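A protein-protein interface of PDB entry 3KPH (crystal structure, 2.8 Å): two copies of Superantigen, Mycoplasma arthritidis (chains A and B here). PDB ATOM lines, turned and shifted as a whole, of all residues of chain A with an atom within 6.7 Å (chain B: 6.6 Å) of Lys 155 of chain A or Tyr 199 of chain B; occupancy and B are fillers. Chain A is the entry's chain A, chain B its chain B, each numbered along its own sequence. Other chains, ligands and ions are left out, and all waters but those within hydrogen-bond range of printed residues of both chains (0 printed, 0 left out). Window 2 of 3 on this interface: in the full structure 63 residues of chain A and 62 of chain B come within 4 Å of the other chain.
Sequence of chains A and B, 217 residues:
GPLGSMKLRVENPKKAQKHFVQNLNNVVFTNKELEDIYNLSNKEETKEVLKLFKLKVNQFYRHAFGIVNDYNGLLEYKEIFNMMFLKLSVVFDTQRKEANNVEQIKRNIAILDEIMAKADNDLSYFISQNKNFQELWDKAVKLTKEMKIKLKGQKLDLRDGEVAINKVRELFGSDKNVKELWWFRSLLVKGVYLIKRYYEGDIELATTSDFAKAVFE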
ATOM      1  N   MET A 147      -5.493  -3.590 -17.661  1.00  0.00           N
ATOM      2  CA  MET A 147      -5.020  -4.383 -16.537  1.00  0.00           C
ATOM      3  C   MET A 147      -4.245  -3.527 -15.561  1.00  0.00           C
ATOM      4  O   MET A 147      -4.099  -3.884 -14.392  1.00  0.00           O
ATOM      5  CB  MET A 147      -4.170  -5.557 -17.023  1.00  0.00           C
ATOM      6  CG  MET A 147      -4.972  -6.595 -17.789  1.00  0.00           C
ATOM      7  SD  MET A 147      -4.021  -8.067 -18.136  1.00  0.00           S
ATOM      8  CE  MET A 147      -3.767  -8.697 -16.473  1.00  0.00           C
ATOM      9  N   LYS A 148      -3.752  -2.388 -16.043  1.00  0.00           N
ATOM     10  CA  LYS A 148      -3.002  -1.480 -15.187  1.00  0.00           C
ATOM     11  C   LYS A 148      -3.978  -1.013 -14.121  1.00  0.00           C
ATOM     12  O   LYS A 148      -3.676  -1.070 -12.929  1.00  0.00           O
ATOM     13  CB  LYS A 148      -2.477  -0.282 -15.976  1.00  0.00           C
ATOM     14  CG  LYS A 148      -1.156   0.274 -15.453  1.00  0.00           C
ATOM     15  CD  LYS A 148      -0.845   1.629 -16.076  1.00  0.00           C
ATOM     16  CE  LYS A 148      -1.043   1.620 -17.577  1.00  0.00           C
ATOM     17  NZ  LYS A 148      -0.936   2.988 -18.139  1.00  0.00           N
ATOM     18  N   ILE A 149      -5.160  -0.576 -14.551  1.00  0.00           N
ATOM     19  CA  ILE A 149      -6.178  -0.113 -13.619  1.00  0.00           C
ATOM     20  C   ILE A 149      -6.724  -1.264 -12.769  1.00  0.00           C
ATOM     21  O   ILE A 149      -6.685  -1.198 -11.544  1.00  0.00           O
ATOM     22  CB  ILE A 149      -7.317   0.586 -14.361  1.00  0.00           C
ATOM     23  CG1 ILE A 149      -6.740   1.609 -15.345  1.00  0.00           C
ATOM     24  CG2 ILE A 149      -8.214   1.284 -13.363  1.00  0.00           C
ATOM     25  CD1 ILE A 149      -7.768   2.215 -16.274  1.00  0.00           C
ATOM     26  N   LYS A 150      -7.199  -2.326 -13.419  1.00  0.00           N
ATOM     27  CA  LYS A 150      -7.754  -3.488 -12.726  1.00  0.00           C
ATOM     28  C   LYS A 150      -6.821  -4.105 -11.687  1.00  0.00           C
ATOM     29  O   LYS A 150      -7.244  -4.426 -10.578  1.00  0.00           O
ATOM     30  CB  LYS A 150      -8.136  -4.568 -13.743  1.00  0.00           C
ATOM     31  CG  LYS A 150      -9.169  -4.162 -14.795  1.00  0.00           C
ATOM     32  CD  LYS A 150     -10.602  -4.306 -14.304  1.00  0.00           C
ATOM     33  CE  LYS A 150     -11.592  -4.284 -15.474  1.00  0.00           C
ATOM     34  NZ  LYS A 150     -11.494  -3.041 -16.296  1.00  0.00           N
ATOM     35  N   LEU A 151      -5.553  -4.281 -12.041  1.00  0.00           N
ATOM     36  CA  LEU A 151      -4.607  -4.895 -11.118  1.00  0.00           C
ATOM     37  C   LEU A 151      -3.939  -3.976 -10.099  1.00  0.00           C
ATOM     38  O   LEU A 151      -3.238  -4.456  -9.200  1.00  0.00           O
ATOM     39  CB  LEU A 151      -3.545  -5.669 -11.904  1.00  0.00           C
ATOM     40  CG  LEU A 151      -3.806  -7.179 -11.946  1.00  0.00           C
ATOM     41  CD1 LEU A 151      -5.289  -7.446 -12.191  1.00  0.00           C
ATOM     42  CD2 LEU A 151      -2.945  -7.822 -13.024  1.00  0.00           C
ATOM     43  N   LYS A 152      -4.170  -2.668 -10.213  1.00  0.00           N
ATOM     44  CA  LYS A 152      -3.559  -1.720  -9.281  1.00  0.00           C
ATOM     45  C   LYS A 152      -3.692  -2.189  -7.837  1.00  0.00           C
ATOM     46  O   LYS A 152      -4.797  -2.313  -7.302  1.00  0.00           O
ATOM     47  CB  LYS A 152      -4.174  -0.328  -9.417  1.00  0.00           C
ATOM     48  CG  LYS A 152      -3.458   0.727  -8.583  1.00  0.00           C
ATOM     49  CD  LYS A 152      -4.307   1.974  -8.398  1.00  0.00           C
ATOM     50  CE  LYS A 152      -4.692   2.595  -9.732  1.00  0.00           C
ATOM     51  NZ  LYS A 152      -5.498   3.831  -9.545  1.00  0.00           N
ATOM     52  N   GLY A 153      -2.547  -2.455  -7.218  1.00  0.00           N
ATOM     53  CA  GLY A 153      -2.533  -2.908  -5.844  1.00  0.00           C
ATOM     54  C   GLY A 153      -3.310  -4.190  -5.620  1.00  0.00           C
ATOM     55  O   GLY A 153      -4.060  -4.301  -4.648  1.00  0.00           O
ATOM     56  N   GLN A 154      -3.147  -5.158  -6.516  1.00  0.00           N
ATOM     57  CA  GLN A 154      -3.836  -6.436  -6.374  1.00  0.00           C
ATOM     58  C   GLN A 154      -2.807  -7.468  -5.952  1.00  0.00           C
ATOM     59  O   GLN A 154      -3.130  -8.634  -5.723  1.00  0.00           O
ATOM     60  CB  GLN A 154      -4.481  -6.867  -7.696  1.00  0.00           C
ATOM     61  CG  GLN A 154      -5.531  -5.905  -8.237  1.00  0.00           C
ATOM     62  CD  GLN A 154      -6.601  -5.540  -7.216  1.00  0.00           C
ATOM     63  OE1 GLN A 154      -7.276  -6.412  -6.668  1.00  0.00           O
ATOM     64  NE2 GLN A 154      -6.763  -4.242  -6.964  1.00  0.00           N
ATOM     65  N   LYS A 155      -1.564  -7.005  -5.847  1.00  0.00           N
ATOM     66  CA  LYS A 155      -0.420  -7.830  -5.475  1.00  0.00           C
ATOM     67  C   LYS A 155      -0.482  -9.233  -6.069  1.00  0.00           C
ATOM     68  O   LYS A 155      -0.476 -10.236  -5.347  1.00  0.00           O
ATOM     69  CB  LYS A 155      -0.265  -7.900  -3.950  1.00  0.00           C
ATOM     70  CG  LYS A 155       1.196  -7.930  -3.511  1.00  0.00           C
ATOM     71  CD  LYS A 155       1.953  -6.753  -4.130  1.00  0.00           C
ATOM     72  CE  LYS A 155       3.462  -6.916  -4.038  1.00  0.00           C
ATOM     73  NZ  LYS A 155       4.153  -5.883  -4.864  1.00  0.00           N
ATOM     74  N   LEU A 156      -0.557  -9.276  -7.399  1.00  0.00           N
ATOM     75  CA  LEU A 156      -0.593 -10.521  -8.164  1.00  0.00           C
ATOM     76  C   LEU A 156       0.829 -11.049  -8.159  1.00  0.00           C
ATOM     77  O   LEU A 156       1.769 -10.291  -8.401  1.00  0.00           O
ATOM     78  CB  LEU A 156      -1.026 -10.247  -9.609  1.00  0.00           C
ATOM     79  CG  LEU A 156      -0.312 -11.031 -10.716  1.00  0.00           C
ATOM     80  CD1 LEU A 156      -0.604 -12.525 -10.600  1.00  0.00           C
ATOM     81  CD2 LEU A 156      -0.762 -10.500 -12.062  1.00  0.00           C
ATOM     82  N   ASP A 157       0.994 -12.342  -7.905  1.00  0.00           N
ATOM     83  CA  ASP A 157       2.336 -12.906  -7.847  1.00  0.00           C
ATOM     84  C   ASP A 157       2.317 -14.417  -8.061  1.00  0.00           C
ATOM     85  O   ASP A 157       2.359 -15.188  -7.101  1.00  0.00           O
ATOM     86  CB  ASP A 157       2.955 -12.573  -6.478  1.00  0.00           C
ATOM     87  CG  ASP A 157       4.480 -12.641  -6.474  1.00  0.00           C
ATOM     88  OD1 ASP A 157       5.125 -11.818  -7.165  1.00  0.00           O
ATOM     89  OD2 ASP A 157       5.035 -13.514  -5.768  1.00  0.00           O
ATOM     90  N   LEU A 158       2.245 -14.837  -9.320  1.00  0.00           N
ATOM     91  CA  LEU A 158       2.238 -16.261  -9.644  1.00  0.00           C
ATOM     92  C   LEU A 158       2.877 -16.524 -11.007  1.00  0.00           C
ATOM     93  O   LEU A 158       2.701 -15.753 -11.953  1.00  0.00           O
ATOM     94  CB  LEU A 158       0.808 -16.820  -9.638  1.00  0.00           C
ATOM     95  CG  LEU A 158       0.003 -17.037  -8.346  1.00  0.00           C
ATOM     96  CD1 LEU A 158       0.831 -17.850  -7.368  1.00  0.00           C
ATOM     97  CD2 LEU A 158      -0.416 -15.706  -7.733  1.00  0.00           C
ATOM     98  N   LEU B 194       4.202  -7.957 -17.444  1.00  0.00           N
ATOM     99  CA  LEU B 194       4.840  -6.663 -17.367  1.00  0.00           C
ATOM    100  C   LEU B 194       4.087  -5.734 -16.431  1.00  0.00           C
ATOM    101  O   LEU B 194       4.708  -5.001 -15.659  1.00  0.00           O
ATOM    102  CB  LEU B 194       5.017  -6.059 -18.767  1.00  0.00           C
ATOM    103  CG  LEU B 194       3.846  -5.495 -19.543  1.00  0.00           C
ATOM    104  CD1 LEU B 194       3.425  -4.182 -18.914  1.00  0.00           C
ATOM    105  CD2 LEU B 194       4.264  -5.270 -20.985  1.00  0.00           C
ATOM    106  N   ILE B 195       2.761  -5.757 -16.464  1.00  0.00           N
ATOM    107  CA  ILE B 195       2.030  -4.895 -15.544  1.00  0.00           C
ATOM    108  C   ILE B 195       2.370  -5.326 -14.118  1.00  0.00           C
ATOM    109  O   ILE B 195       2.468  -4.493 -13.219  1.00  0.00           O
ATOM    110  CB  ILE B 195       0.520  -4.941 -15.815  1.00  0.00           C
ATOM    111  CG1 ILE B 195       0.212  -3.936 -16.922  1.00  0.00           C
ATOM    112  CG2 ILE B 195      -0.273  -4.628 -14.559  1.00  0.00           C
ATOM    113  CD1 ILE B 195      -1.065  -4.193 -17.633  1.00  0.00           C
ATOM    114  N   LYS B 196       2.581  -6.623 -13.917  1.00  0.00           N
ATOM    115  CA  LYS B 196       2.954  -7.119 -12.601  1.00  0.00           C
ATOM    116  C   LYS B 196       4.289  -6.503 -12.218  1.00  0.00           C
ATOM    117  O   LYS B 196       4.465  -6.030 -11.097  1.00  0.00           O
ATOM    118  CB  LYS B 196       3.117  -8.635 -12.605  1.00  0.00           C
ATOM    119  CG  LYS B 196       3.851  -9.137 -11.375  1.00  0.00           C
ATOM    120  CD  LYS B 196       4.144 -10.619 -11.444  1.00  0.00           C
ATOM    121  CE  LYS B 196       4.816 -11.097 -10.160  1.00  0.00           C
ATOM    122  NZ  LYS B 196       4.978 -12.583 -10.112  1.00  0.00           N
ATOM    123  N   ARG B 197       5.236  -6.532 -13.154  1.00  0.00           N
ATOM    124  CA  ARG B 197       6.561  -5.964 -12.921  1.00  0.00           C
ATOM    125  C   ARG B 197       6.397  -4.495 -12.587  1.00  0.00           C
ATOM    126  O   ARG B 197       6.952  -4.002 -11.608  1.00  0.00           O
ATOM    127  CB  ARG B 197       7.440  -6.110 -14.165  1.00  0.00           C
ATOM    128  CG  ARG B 197       7.993  -7.511 -14.394  1.00  0.00           C
ATOM    129  CD  ARG B 197       8.974  -7.500 -15.560  1.00  0.00           C
ATOM    130  NE  ARG B 197      10.211  -8.229 -15.270  1.00  0.00           N
ATOM    131  CZ  ARG B 197      11.019  -7.976 -14.239  1.00  0.00           C
ATOM    132  NH1 ARG B 197      12.123  -8.696 -14.067  1.00  0.00           N
ATOM    133  NH2 ARG B 197      10.726  -7.011 -13.372  1.00  0.00           N
ATOM    134  N   TYR B 198       5.616  -3.807 -13.411  1.00  0.00           N
ATOM    135  CA  TYR B 198       5.349  -2.400 -13.214  1.00  0.00           C
ATOM    136  C   TYR B 198       4.977  -2.131 -11.762  1.00  0.00           C
ATOM    137  O   TYR B 198       5.595  -1.295 -11.108  1.00  0.00           O
ATOM    138  CB  TYR B 198       4.211  -1.964 -14.120  1.00  0.00           C
ATOM    139  CG  TYR B 198       3.855  -0.515 -13.968  1.00  0.00           C
ATOM    140  CD1 TYR B 198       4.701   0.479 -14.445  1.00  0.00           C
ATOM    141  CD2 TYR B 198       2.664  -0.135 -13.354  1.00  0.00           C
ATOM    142  CE1 TYR B 198       4.370   1.822 -14.320  1.00  0.00           C
ATOM    143  CE2 TYR B 198       2.324   1.202 -13.221  1.00  0.00           C
ATOM    144  CZ  TYR B 198       3.179   2.174 -13.709  1.00  0.00           C
ATOM    145  OH  TYR B 198       2.832   3.499 -13.604  1.00  0.00           O
ATOM    146  N   TYR B 199       3.980  -2.848 -11.248  1.00  0.00           N
ATOM    147  CA  TYR B 199       3.556  -2.641  -9.869  1.00  0.00           C
ATOM    148  C   TYR B 199       4.459  -3.258  -8.817  1.00  0.00           C
ATOM    149  O   TYR B 199       4.123  -3.294  -7.633  1.00  0.00           O
ATOM    150  CB  TYR B 199       2.102  -3.083  -9.682  1.00  0.00           C
ATOM    151  CG  TYR B 199       1.150  -2.036 -10.203  1.00  0.00           C
ATOM    152  CD1 TYR B 199      -0.028  -2.387 -10.843  1.00  0.00           C
ATOM    153  CD2 TYR B 199       1.467  -0.684 -10.112  1.00  0.00           C
ATOM    154  CE1 TYR B 199      -0.862  -1.415 -11.391  1.00  0.00           C
ATOM    155  CE2 TYR B 199       0.644   0.291 -10.652  1.00  0.00           C
ATOM    156  CZ  TYR B 199      -0.517  -0.079 -11.294  1.00  0.00           C
ATOM    157  OH  TYR B 199      -1.323   0.881 -11.864  1.00  0.00           O
ATOM    158  N   GLU B 200       5.615  -3.740  -9.245  1.00  0.00           N
ATOM    159  CA  GLU B 200       6.570  -4.285  -8.300  1.00  0.00           C
ATOM    160  C   GLU B 200       7.734  -3.306  -8.312  1.00  0.00           C
ATOM    161  O   GLU B 200       8.858  -3.647  -7.942  1.00  0.00           O
ATOM    162  CB  GLU B 200       7.016  -5.689  -8.718  1.00  0.00           C
ATOM    163  CG  GLU B 200       5.912  -6.730  -8.571  1.00  0.00           C
ATOM    164  CD  GLU B 200       6.363  -8.131  -8.930  1.00  0.00           C
ATOM    165  OE1 GLU B 200       6.915  -8.301 -10.039  1.00  0.00           O
ATOM    166  OE2 GLU B 200       6.163  -9.056  -8.111  1.00  0.00           O
ATOM    167  N   GLY B 201       7.435  -2.074  -8.732  1.00  0.00           N
ATOM    168  CA  GLY B 201       8.447  -1.036  -8.804  1.00  0.00           C
ATOM    169  C   GLY B 201       9.405  -1.381  -9.922  1.00  0.00           C
ATOM    170  O   GLY B 201      10.237  -2.277  -9.778  1.00  0.00           O
ATOM    171  N   ASP B 202       9.307  -0.676 -11.040  1.00  0.00           N
ATOM    172  CA  ASP B 202      10.169  -0.999 -12.152  1.00  0.00           C
ATOM    173  C   ASP B 202      10.299   0.134 -13.152  1.00  0.00           C
ATOM    174  O   ASP B 202      11.311   0.836 -13.198  1.00  0.00           O
ATOM    175  CB  ASP B 202       9.600  -2.234 -12.851  1.00  0.00           C
ATOM    176  CG  ASP B 202      10.658  -3.247 -13.218  1.00  0.00           C
ATOM    177  OD1 ASP B 202      11.524  -2.929 -14.055  1.00  0.00           O
ATOM    178  OD2 ASP B 202      10.614  -4.367 -12.666  1.00  0.00           O
ATOM    179  N   LEU B 205      10.254   0.325 -18.289  1.00  0.00           N
ATOM    180  CA  LEU B 205       9.687  -0.781 -19.045  1.00  0.00           C
ATOM    181  C   LEU B 205       9.127  -0.283 -20.365  1.00  0.00           C
ATOM    182  O   LEU B 205       9.076  -1.023 -21.343  1.00  0.00           O
ATOM    183  CB  LEU B 205       8.588  -1.469 -18.233  1.00  0.00           C
ATOM    184  CG  LEU B 205       9.047  -2.583 -17.293  1.00  0.00           C
ATOM    185  CD1 LEU B 205      10.193  -2.107 -16.441  1.00  0.00           C
ATOM    186  CD2 LEU B 205       7.890  -3.025 -16.432  1.00  0.00           C
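O of Lys 148 of chain A lies close to OH of Tyr 199 of chain B (3.2 Å). OD1 of Asp 157 of chain A lies within salt-bridge range of NZ of Lys 196 of chain B (3.0 Å). The side-chain carboxylate (OE2) of Glu 200 of chain B lies close to the side-chain carboxylate (OD1) of Asp 157 of chain A, 3.1 Å away.
No position is printed for both chains. Of the 9 pairs that touch across the chains among the printed residues, none has its exchanged pair printed and touching as well.
Lys 155 of chain A touches just one residue of chain B: Tyr 199 (3.8 Å). Tyr 199 of chain B touches just these residues of chain A: Lys 148, Lys 152 and Lys 155. Of the printed residues of chain A, Glu 200 of chain B touches Asp 157 (3.1 Å). Of the printed residues of chain B, Met 147 of chain A touches Ile 195. Leu 194 of chain B touches none of the printed residues of chain A. The nearest residue of chain B that does not touch Lys 155 of chain A is Glu 200 of chain B (4.2 Å). The nearest residue of chain A that does not touch Tyr 199 of chain B is Leu 151 of chain A (4.2 Å).
Of the 10 printed residues of chain B, 4 touch a printed residue of chain A. Along chain B the printed residues that touch a printed residue of chain A span positions 195 to 200. Hydrophobic or aromatic side chains of chain A that line the printed part of chain B: Met 147. Among the printed residues, Asp or Glu carboxylates within 4 Å of a Lys or Arg side-chain nitrogen of the other chain: Asp 157 of chain A with Lys 196 of chain B (3.0 Å).
Among the printed residues, pairs that only touch across the chains: Lys 152 of chain A with Tyr 199 of chain B, Met 147 of chain A with Ile 195 of chain B, Lys 148 of chain A with Ile 195 of chain B, Leu 156 of chain A with Lys 196 of chain B, Leu 158 of chain A with Lys 196 of chain B and Lys 155 of chain A with Tyr 199 of chain B.
The side-chain amide nitrogen (NE2) of Gln 154 of chain A is in hydrogen-bond range of the backbone carbonyl oxygen (O) of Lys 152 of chain A, 2.8 Å away.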
